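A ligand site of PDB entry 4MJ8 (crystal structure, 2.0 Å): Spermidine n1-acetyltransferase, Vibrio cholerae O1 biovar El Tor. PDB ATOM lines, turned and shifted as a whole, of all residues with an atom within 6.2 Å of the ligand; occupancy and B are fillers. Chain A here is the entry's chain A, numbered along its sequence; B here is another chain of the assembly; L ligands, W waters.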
ATOM      1  N   ASN A  25     -21.218   1.890 -31.851  1.00  0.00           N
ATOM      2  CA  ASN A  25     -21.618   2.577 -30.611  1.00  0.00           C
ATOM      3  C   ASN A  25     -22.244   3.934 -30.805  1.00  0.00           C
ATOM      4  O   ASN A  25     -22.881   4.474 -29.868  1.00  0.00           O
ATOM      5  CB  ASN A  25     -20.443   2.642 -29.609  1.00  0.00           C
ATOM      6  CG  ASN A  25     -20.096   1.263 -29.048  1.00  0.00           C
ATOM      7  OD1 ASN A  25     -20.698   0.251 -29.421  1.00  0.00           O
ATOM      8  ND2 ASN A  25     -19.133   1.230 -28.142  1.00  0.00           N
ATOM      9  N   MET A  31     -27.483   0.556 -31.212  1.00  0.00           N
ATOM     10  CA  MET A  31     -27.438   0.646 -29.763  1.00  0.00           C
ATOM     11  C   MET A  31     -28.798   0.458 -29.016  1.00  0.00           C
ATOM     12  O   MET A  31     -28.810   0.155 -27.810  1.00  0.00           O
ATOM     13  CB  MET A  31     -26.756   1.960 -29.374  1.00  0.00           C
ATOM     14  CG  MET A  31     -25.252   2.001 -29.561  1.00  0.00           C
ATOM     15  SD  MET A  31     -24.328   0.851 -28.517  1.00  0.00           S
ATOM     16  CE  MET A  31     -24.083  -0.534 -29.571  1.00  0.00           C
ATOM     17  N   TRP A  34     -29.153  -2.862 -27.366  1.00  0.00           N
ATOM     18  CA  TRP A  34     -28.469  -3.044 -26.130  1.00  0.00           C
ATOM     19  C   TRP A  34     -28.947  -2.099 -25.003  1.00  0.00           C
ATOM     20  O   TRP A  34     -28.367  -2.110 -23.912  1.00  0.00           O
ATOM     21  CB  TRP A  34     -26.970  -2.916 -26.321  1.00  0.00           C
ATOM     22  CG  TRP A  34     -26.345  -4.093 -26.875  1.00  0.00           C
ATOM     23  CD1 TRP A  34     -26.951  -5.122 -27.584  1.00  0.00           C
ATOM     24  CD2 TRP A  34     -24.963  -4.317 -26.934  1.00  0.00           C
ATOM     25  NE1 TRP A  34     -26.010  -5.999 -27.988  1.00  0.00           N
ATOM     26  CE2 TRP A  34     -24.770  -5.535 -27.616  1.00  0.00           C
ATOM     27  CE3 TRP A  34     -23.846  -3.633 -26.448  1.00  0.00           C
ATOM     28  CZ2 TRP A  34     -23.508  -6.072 -27.830  1.00  0.00           C
ATOM     29  CZ3 TRP A  34     -22.592  -4.165 -26.664  1.00  0.00           C
ATOM     30  CH2 TRP A  34     -22.433  -5.375 -27.332  1.00  0.00           C
ATOM     31  N   GLU A  36     -28.723   1.040 -24.883  1.00  0.00           N
ATOM     32  CA  GLU A  36     -27.651   1.992 -24.586  1.00  0.00           C
ATOM     33  C   GLU A  36     -27.739   3.244 -25.411  1.00  0.00           C
ATOM     34  O   GLU A  36     -28.349   3.262 -26.507  1.00  0.00           O
ATOM     35  CB  GLU A  36     -26.260   1.309 -24.579  1.00  0.00           C
ATOM     36  CG  GLU A  36     -26.133   0.400 -23.350  1.00  0.00           C
ATOM     37  CD  GLU A  36     -24.811  -0.301 -23.173  1.00  0.00           C
ATOM     38  OE1 GLU A  36     -23.760   0.360 -23.338  1.00  0.00           O
ATOM     39  OE2 GLU A  36     -24.813  -1.496 -22.803  1.00  0.00           O
ATOM     40  N   GLU A  37     -27.215   4.310 -24.829  1.00  0.00           N
ATOM     41  CA  GLU A  37     -27.243   5.626 -25.442  1.00  0.00           C
ATOM     42  C   GLU A  37     -26.263   5.589 -26.627  1.00  0.00           C
ATOM     43  O   GLU A  37     -25.095   5.192 -26.405  1.00  0.00           O
ATOM     44  CB  GLU A  37     -26.795   6.701 -24.397  1.00  0.00           C
ATOM     45  CG  GLU A  37     -26.761   8.074 -25.021  1.00  0.00           C
ATOM     46  CD  GLU A  37     -26.217   9.187 -24.153  1.00  0.00           C
ATOM     47  OE1 GLU A  37     -26.108  10.329 -24.685  1.00  0.00           O
ATOM     48  OE2 GLU A  37     -25.902   8.955 -22.971  1.00  0.00           O
ATOM     49  N   PRO A  38     -26.673   6.023 -27.832  1.00  0.00           N
ATOM     50  CA  PRO A  38     -25.757   5.988 -28.987  1.00  0.00           C
ATOM     51  C   PRO A  38     -24.831   7.232 -29.142  1.00  0.00           C
ATOM     52  O   PRO A  38     -24.875   7.965 -30.147  1.00  0.00           O
ATOM     53  CB  PRO A  38     -26.743   5.903 -30.158  1.00  0.00           C
ATOM     54  CG  PRO A  38     -27.871   6.822 -29.708  1.00  0.00           C
ATOM     55  CD  PRO A  38     -28.013   6.471 -28.239  1.00  0.00           C
ATOM     56  N   TYR A  39     -24.000   7.451 -28.155  1.00  0.00           N
ATOM     57  CA  TYR A  39     -23.046   8.559 -28.158  1.00  0.00           C
ATOM     58  C   TYR A  39     -21.828   8.086 -27.396  1.00  0.00           C
ATOM     59  O   TYR A  39     -21.900   7.717 -26.219  1.00  0.00           O
ATOM     60  CB  TYR A  39     -23.627   9.801 -27.435  1.00  0.00           C
ATOM     61  CG  TYR A  39     -22.692  10.996 -27.363  1.00  0.00           C
ATOM     62  CD1 TYR A  39     -21.536  10.984 -26.575  1.00  0.00           C
ATOM     63  CD2 TYR A  39     -23.023  12.171 -27.996  1.00  0.00           C
ATOM     64  CE1 TYR A  39     -20.688  12.058 -26.515  1.00  0.00           C
ATOM     65  CE2 TYR A  39     -22.176  13.258 -27.946  1.00  0.00           C
ATOM     66  CZ  TYR A  39     -21.026  13.205 -27.199  1.00  0.00           C
ATOM     67  OH  TYR A  39     -20.220  14.332 -27.178  1.00  0.00           O
ATOM     68  N   GLU A  40     -20.702   8.037 -28.086  1.00  0.00           N
ATOM     69  CA  GLU A  40     -19.509   7.737 -27.374  1.00  0.00           C
ATOM     70  C   GLU A  40     -18.347   8.240 -28.176  1.00  0.00           C
ATOM     71  O   GLU A  40     -18.092   7.739 -29.305  1.00  0.00           O
ATOM     72  CB  GLU A  40     -19.381   6.249 -27.145  1.00  0.00           C
ATOM     73  CG  GLU A  40     -18.195   5.884 -26.300  1.00  0.00           C
ATOM     74  CD  GLU A  40     -18.134   4.395 -25.981  1.00  0.00           C
ATOM     75  OE1 GLU A  40     -17.933   4.044 -24.786  1.00  0.00           O
ATOM     76  OE2 GLU A  40     -18.278   3.607 -26.919  1.00  0.00           O
ATOM     77  N   SER A  41     -17.615   9.227 -27.626  1.00  0.00           N
ATOM     78  CA  SER A  41     -16.429   9.675 -28.361  1.00  0.00           C
ATOM     79  C   SER A  41     -15.407   8.555 -28.438  1.00  0.00           C
ATOM     80  O   SER A  41     -15.369   7.627 -27.601  1.00  0.00           O
ATOM     81  CB  SER A  41     -15.756  10.893 -27.747  1.00  0.00           C
ATOM     82  OG  SER A  41     -15.108  10.503 -26.572  1.00  0.00           O
ATOM     83  N   GLU A  44     -13.609   8.237 -25.147  1.00  0.00           N
ATOM     84  CA  GLU A  44     -14.289   7.588 -24.041  1.00  0.00           C
ATOM     85  C   GLU A  44     -14.172   6.074 -24.260  1.00  0.00           C
ATOM     86  O   GLU A  44     -13.813   5.308 -23.370  1.00  0.00           O
ATOM     87  CB  GLU A  44     -15.768   8.033 -23.934  1.00  0.00           C
ATOM     88  CG  GLU A  44     -16.514   7.283 -22.816  1.00  0.00           C
ATOM     89  CD  GLU A  44     -17.963   7.722 -22.582  1.00  0.00           C
ATOM     90  OE1 GLU A  44     -18.526   7.213 -21.611  1.00  0.00           O
ATOM     91  OE2 GLU A  44     -18.537   8.524 -23.299  1.00  0.00           O
ATOM     92  N   LEU A  48     -12.069   3.677 -21.767  1.00  0.00           N
ATOM     93  CA  LEU A  48     -12.795   2.596 -21.073  1.00  0.00           C
ATOM     94  C   LEU A  48     -12.202   1.249 -21.465  1.00  0.00           C
ATOM     95  O   LEU A  48     -12.070   0.379 -20.613  1.00  0.00           O
ATOM     96  CB  LEU A  48     -14.289   2.620 -21.333  1.00  0.00           C
ATOM     97  CG  LEU A  48     -14.999   3.816 -20.652  1.00  0.00           C
ATOM     98  CD1 LEU A  48     -16.415   3.825 -21.172  1.00  0.00           C
ATOM     99  CD2 LEU A  48     -15.055   3.817 -19.097  1.00  0.00           C
ATOM    100  N   ARG A  60     -14.935  -9.610 -24.199  1.00  0.00           N
ATOM    101  CA  ARG A  60     -15.459  -8.940 -25.411  1.00  0.00           C
ATOM    102  C   ARG A  60     -14.851  -9.531 -26.667  1.00  0.00           C
ATOM    103  O   ARG A  60     -13.642  -9.644 -26.771  1.00  0.00           O
ATOM    104  CB  ARG A  60     -15.169  -7.453 -25.332  1.00  0.00           C
ATOM    105  CG  ARG A  60     -15.848  -6.753 -24.153  1.00  0.00           C
ATOM    106  CD  ARG A  60     -15.487  -5.286 -24.071  1.00  0.00           C
ATOM    107  NE  ARG A  60     -16.110  -4.543 -25.150  1.00  0.00           N
ATOM    108  CZ  ARG A  60     -15.927  -3.260 -25.368  1.00  0.00           C
ATOM    109  NH1 ARG A  60     -15.097  -2.562 -24.599  1.00  0.00           N
ATOM    110  NH2 ARG A  60     -16.560  -2.681 -26.374  1.00  0.00           N
ATOM    111  N   HIS B  52     -12.937  16.543 -19.578  1.00  0.00           N
ATOM    112  CA  HIS B  52     -14.360  16.199 -19.611  1.00  0.00           C
ATOM    113  C   HIS B  52     -14.793  14.964 -20.405  1.00  0.00           C
ATOM    114  O   HIS B  52     -15.990  14.777 -20.595  1.00  0.00           O
ATOM    115  CB  HIS B  52     -15.191  17.446 -20.092  1.00  0.00           C
ATOM    116  CG  HIS B  52     -15.166  18.561 -19.084  1.00  0.00           C
ATOM    117  ND1 HIS B  52     -15.988  18.578 -17.972  1.00  0.00           N
ATOM    118  CD2 HIS B  52     -14.320  19.618 -18.942  1.00  0.00           C
ATOM    119  CE1 HIS B  52     -15.683  19.636 -17.226  1.00  0.00           C
ATOM    120  NE2 HIS B  52     -14.682  20.278 -17.797  1.00  0.00           N
ATOM    121  N   ILE B  53     -13.870  14.107 -20.772  1.00  0.00           N
ATOM    122  CA  ILE B  53     -14.174  12.936 -21.586  1.00  0.00           C
ATOM    123  C   ILE B  53     -15.271  12.128 -20.997  1.00  0.00           C
ATOM    124  O   ILE B  53     -16.233  11.776 -21.688  1.00  0.00           O
ATOM    125  CB  ILE B  53     -12.908  12.060 -21.870  1.00  0.00           C
ATOM    126  CG1 ILE B  53     -12.008  12.829 -22.798  1.00  0.00           C
ATOM    127  CG2 ILE B  53     -13.312  10.699 -22.483  1.00  0.00           C
ATOM    128  CD1 ILE B  53     -10.630  12.244 -23.021  1.00  0.00           C
ATOM    129  N   HIS B  54     -15.192  11.925 -19.686  1.00  0.00           N
ATOM    130  CA  HIS B  54     -16.150  11.104 -18.990  1.00  0.00           C
ATOM    131  C   HIS B  54     -17.198  11.876 -18.206  1.00  0.00           C
ATOM    132  O   HIS B  54     -17.910  11.288 -17.463  1.00  0.00           O
ATOM    133  CB  HIS B  54     -15.394  10.126 -18.063  1.00  0.00           C
ATOM    134  CG  HIS B  54     -14.349   9.338 -18.766  1.00  0.00           C
ATOM    135  ND1 HIS B  54     -14.625   8.175 -19.453  1.00  0.00           N
ATOM    136  CD2 HIS B  54     -13.010   9.522 -18.876  1.00  0.00           C
ATOM    137  CE1 HIS B  54     -13.515   7.684 -19.960  1.00  0.00           C
ATOM    138  NE2 HIS B  54     -12.530   8.501 -19.654  1.00  0.00           N
ATOM    139  N   ASP B  55     -17.292  13.176 -18.424  1.00  0.00           N
ATOM    140  CA  ASP B  55     -18.258  13.997 -17.707  1.00  0.00           C
ATOM    141  C   ASP B  55     -19.660  13.743 -18.288  1.00  0.00           C
ATOM    142  O   ASP B  55     -19.953  14.054 -19.447  1.00  0.00           O
ATOM    143  CB  ASP B  55     -17.854  15.425 -17.910  1.00  0.00           C
ATOM    144  CG  ASP B  55     -18.768  16.402 -17.199  1.00  0.00           C
ATOM    145  OD1 ASP B  55     -19.755  15.993 -16.561  1.00  0.00           O
ATOM    146  OD2 ASP B  55     -18.459  17.588 -17.331  1.00  0.00           O
ATOM    147  N   ASN B  56     -20.503  13.115 -17.496  1.00  0.00           N
ATOM    148  CA  ASN B  56     -21.845  12.750 -17.889  1.00  0.00           C
ATOM    149  C   ASN B  56     -22.816  13.921 -17.967  1.00  0.00           C
ATOM    150  O   ASN B  56     -23.934  13.758 -18.478  1.00  0.00           O
ATOM    151  CB  ASN B  56     -22.403  11.729 -16.882  1.00  0.00           C
ATOM    152  CG  ASN B  56     -23.631  10.996 -17.387  1.00  0.00           C
ATOM    153  OD1 ASN B  56     -24.618  10.745 -16.663  1.00  0.00           O
ATOM    154  ND2 ASN B  56     -23.565  10.611 -18.645  1.00  0.00           N
ATOM    155  N   ALA B  57     -22.394  15.091 -17.447  1.00  0.00           N
ATOM    156  CA  ALA B  57     -23.263  16.294 -17.395  1.00  0.00           C
ATOM    157  C   ALA B  57     -23.331  17.103 -18.702  1.00  0.00           C
ATOM    158  O   ALA B  57     -23.950  18.173 -18.764  1.00  0.00           O
ATOM    159  CB  ALA B  57     -22.848  17.180 -16.239  1.00  0.00           C
ATOM    160  N   GLU B  58     -22.644  16.610 -19.743  1.00  0.00           N
ATOM    161  CA  GLU B  58     -22.663  17.280 -21.017  1.00  0.00           C
ATOM    162  C   GLU B  58     -22.633  16.342 -22.163  1.00  0.00           C
ATOM    163  O   GLU B  58     -22.122  15.229 -22.058  1.00  0.00           O
ATOM    164  CB  GLU B  58     -21.417  18.209 -21.185  1.00  0.00           C
ATOM    165  CG  GLU B  58     -20.060  17.512 -21.174  1.00  0.00           C
ATOM    166  CD  GLU B  58     -18.869  18.495 -21.436  1.00  0.00           C
ATOM    167  OE1 GLU B  58     -18.856  19.557 -20.835  1.00  0.00           O
ATOM    168  OE2 GLU B  58     -17.958  18.199 -22.249  1.00  0.00           O
ATOM    169  N   ARG B  59     -23.171  16.825 -23.290  1.00  0.00           N
ATOM    170  CA  ARG B  59     -23.036  16.114 -24.546  1.00  0.00           C
ATOM    171  C   ARG B  59     -22.700  17.183 -25.605  1.00  0.00           C
ATOM    172  O   ARG B  59     -23.535  18.083 -25.843  1.00  0.00           O
ATOM    173  CB  ARG B  59     -24.315  15.383 -24.969  1.00  0.00           C
ATOM    174  CG  ARG B  59     -24.761  14.187 -24.119  1.00  0.00           C
ATOM    175  CD  ARG B  59     -23.811  12.999 -24.106  1.00  0.00           C
ATOM    176  NE  ARG B  59     -24.356  11.957 -23.238  1.00  0.00           N
ATOM    177  CZ  ARG B  59     -24.293  11.904 -21.914  1.00  0.00           C
ATOM    178  NH1 ARG B  59     -24.895  10.918 -21.302  1.00  0.00           N
ATOM    179  NH2 ARG B  59     -23.652  12.817 -21.205  1.00  0.00           N
ATOM    180  N   ARG B  60     -21.559  17.042 -26.300  1.00  0.00           N
ATOM    181  CA  ARG B  60     -21.162  18.011 -27.324  1.00  0.00           C
ATOM    182  C   ARG B  60     -21.217  17.304 -28.635  1.00  0.00           C
ATOM    183  O   ARG B  60     -20.633  16.190 -28.781  1.00  0.00           O
ATOM    184  CB  ARG B  60     -19.763  18.491 -27.036  1.00  0.00           C
ATOM    185  CG  ARG B  60     -19.662  19.091 -25.632  1.00  0.00           C
ATOM    186  CD  ARG B  60     -18.215  19.508 -25.364  1.00  0.00           C
ATOM    187  NE  ARG B  60     -17.822  20.615 -26.169  1.00  0.00           N
ATOM    188  CZ  ARG B  60     -16.590  21.129 -26.196  1.00  0.00           C
ATOM    189  NH1 ARG B  60     -15.585  20.560 -25.520  1.00  0.00           N
ATOM    190  NH2 ARG B  60     -16.365  22.217 -26.940  1.00  0.00           N
HETATM  191  N1  LIG L   1     -18.487  13.677 -21.866  1.00  0.00           N
HETATM  192  C1  LIG L   1     -19.464  12.930 -22.650  1.00  0.00           C
HETATM  193  C2  LIG L   1     -19.684  11.598 -21.980  1.00  0.00           C
HETATM  194  C3  LIG L   1     -20.610  10.791 -22.854  1.00  0.00           C
HETATM  195  N2  LIG L   1     -20.916   9.489 -22.322  1.00  0.00           N
HETATM  196  C4  LIG L   1     -22.023   8.770 -22.907  1.00  0.00           C
HETATM  197  C5  LIG L   1     -21.812   7.272 -22.886  1.00  0.00           C
HETATM  198  C6  LIG L   1     -23.136   6.662 -23.300  1.00  0.00           C
HETATM  199  C7  LIG L   1     -23.179   5.173 -23.060  1.00  0.00           C
HETATM  200  N3  LIG L   1     -22.226   4.501 -23.896  1.00  0.00           N
HETATM  201  C8  LIG L   1     -22.020   3.067 -23.765  1.00  0.00           C
HETATM  202  C9  LIG L   1     -20.882   2.604 -24.685  1.00  0.00           C
HETATM  203  C10 LIG L   1     -21.069   1.170 -25.175  1.00  0.00           C
HETATM  204  N4  LIG L   1     -22.198   1.151 -26.079  1.00  0.00           N
HETATM  205  O   HOH W   1     -18.364  10.331 -25.232  1.00  0.00           O
HETATM  206  O   HOH W   2     -19.812  -2.065 -25.504  1.00  0.00           O
HETATM  207  O   HOH W   3     -22.791   3.835 -27.342  1.00  0.00           O
HETATM  208  O   HOH W   4     -19.431   4.904 -22.845  1.00  0.00           O
HETATM  209  O   HOH W   5     -18.076  -0.356 -26.075  1.00  0.00           O
HETATM  210  O   HOH W   6     -21.346   9.736 -19.795  1.00  0.00           O
HETATM  211  O   HOH W   7     -26.164   4.365 -21.907  1.00  0.00           O
HETATM  212  O   HOH W   8     -19.585  15.550 -24.681  1.00  0.00           O
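Asn 25 touches the ligand.
Glu 37 touches the ligand.
Tyr 39 touches the ligand (O to C6, 3.3 Å).
OE1 of Glu 40 touches C9 of the ligand, 3.3 Å away.
Glu 58 of chain B touches the ligand.
NH1 of Arg 59 of chain B touches C4 of the ligand, at 3.9 Å.
Hydrophobic or aromatic side chains that line the ligand: Met 31 and Tyr 39.
Within 4 Å of the ligand: Asn 25, Met 31, Glu 36, Glu 37, Tyr 39, Glu 40, Glu 44, His 52 of chain B, Ile 53 of chain B, Asp 55 of chain B, Glu 58 of chain B and Arg 59 of chain B.
Along chain A the residues within 4 Å of the ligand span positions 25 to 44.
The nearest printed residue that does not touch the ligand is His 54 of chain B (4.3 Å).
SD of Met 31 is in hydrogen-bond range of N4 of the ligand, at 3.3 Å.
O of Asp 55 of chain B is in hydrogen-bond range of N1 of the ligand, 2.9 Å away.
The backbone carbonyl oxygen (O) of His 52 of chain B lies within hydrogen-bond range of a nitrogen (N1) of the ligand (3.0 Å).
N2 of the ligand is in salt-bridge range of OE2 of Glu 44 (2.7 Å).
N1 of the ligand is in hydrogen-bond range of O of Ile 53 of chain B (3.0 Å).
OE1 of Glu 36 is in salt-bridge range of N4 of the ligand (3.3 Å).
Water W6 lies within hydrogen-bond range of a nitrogen (N2) of the ligand (2.6 Å) and the side-chain amide nitrogen (ND2) of Asn 56 of chain B (2.6 Å).
Water W4 lies within hydrogen-bond range of OE1 of Glu 40, OE1 of Glu 44 and N3 of the ligand.
Water W1 lies within hydrogen-bond range of the side-chain carboxylate of Glu 44 (2.7 Å) and the backbone NH of Ser 41 (2.7 Å).
Water W8 bridges OH of Tyr 39 (2.8 Å) and N of Arg 60 of chain B (3.0 Å).
Water W5 lies within hydrogen-bond range of NH2 of Arg 60 of chain A (2.8 Å) and ND2 of Asn 25 (2.8 Å).
The side-chain hydroxyl (OH) of Tyr 39 is in hydrogen-bond range of the backbone carbonyl oxygen (O) of Arg 60 of chain B (2.5 Å).
SD of Met 31 sits close to OD1 of Asn 25, 3.8 Å away.
N of Glu 44 sits at hydrogen-bond distance from OG of Ser 41, at 3.1 Å.
O of Met 31 sits at hydrogen-bond distance from N of Glu 36, 3.1 Å away.
The backbone carbonyl oxygen (O) of Asn 56 of chain B lies within hydrogen-bond range of the guanidinium group (NH2) of Arg 59 of chain B, at 2.9 Å.
The side-chain carboxylate of Glu 40 lies within hydrogen-bond range of the side-chain amide nitrogen of Asn 25 (2.8 Å).
NH1 of Arg 59 of chain B is in salt-bridge range of OE2 of Glu 37 (2.8 Å).
The side-chain carboxylate (OD2) of Asp 55 of chain B lies within hydrogen-bond range of a ring nitrogen (ND1) of His 52 of chain B.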
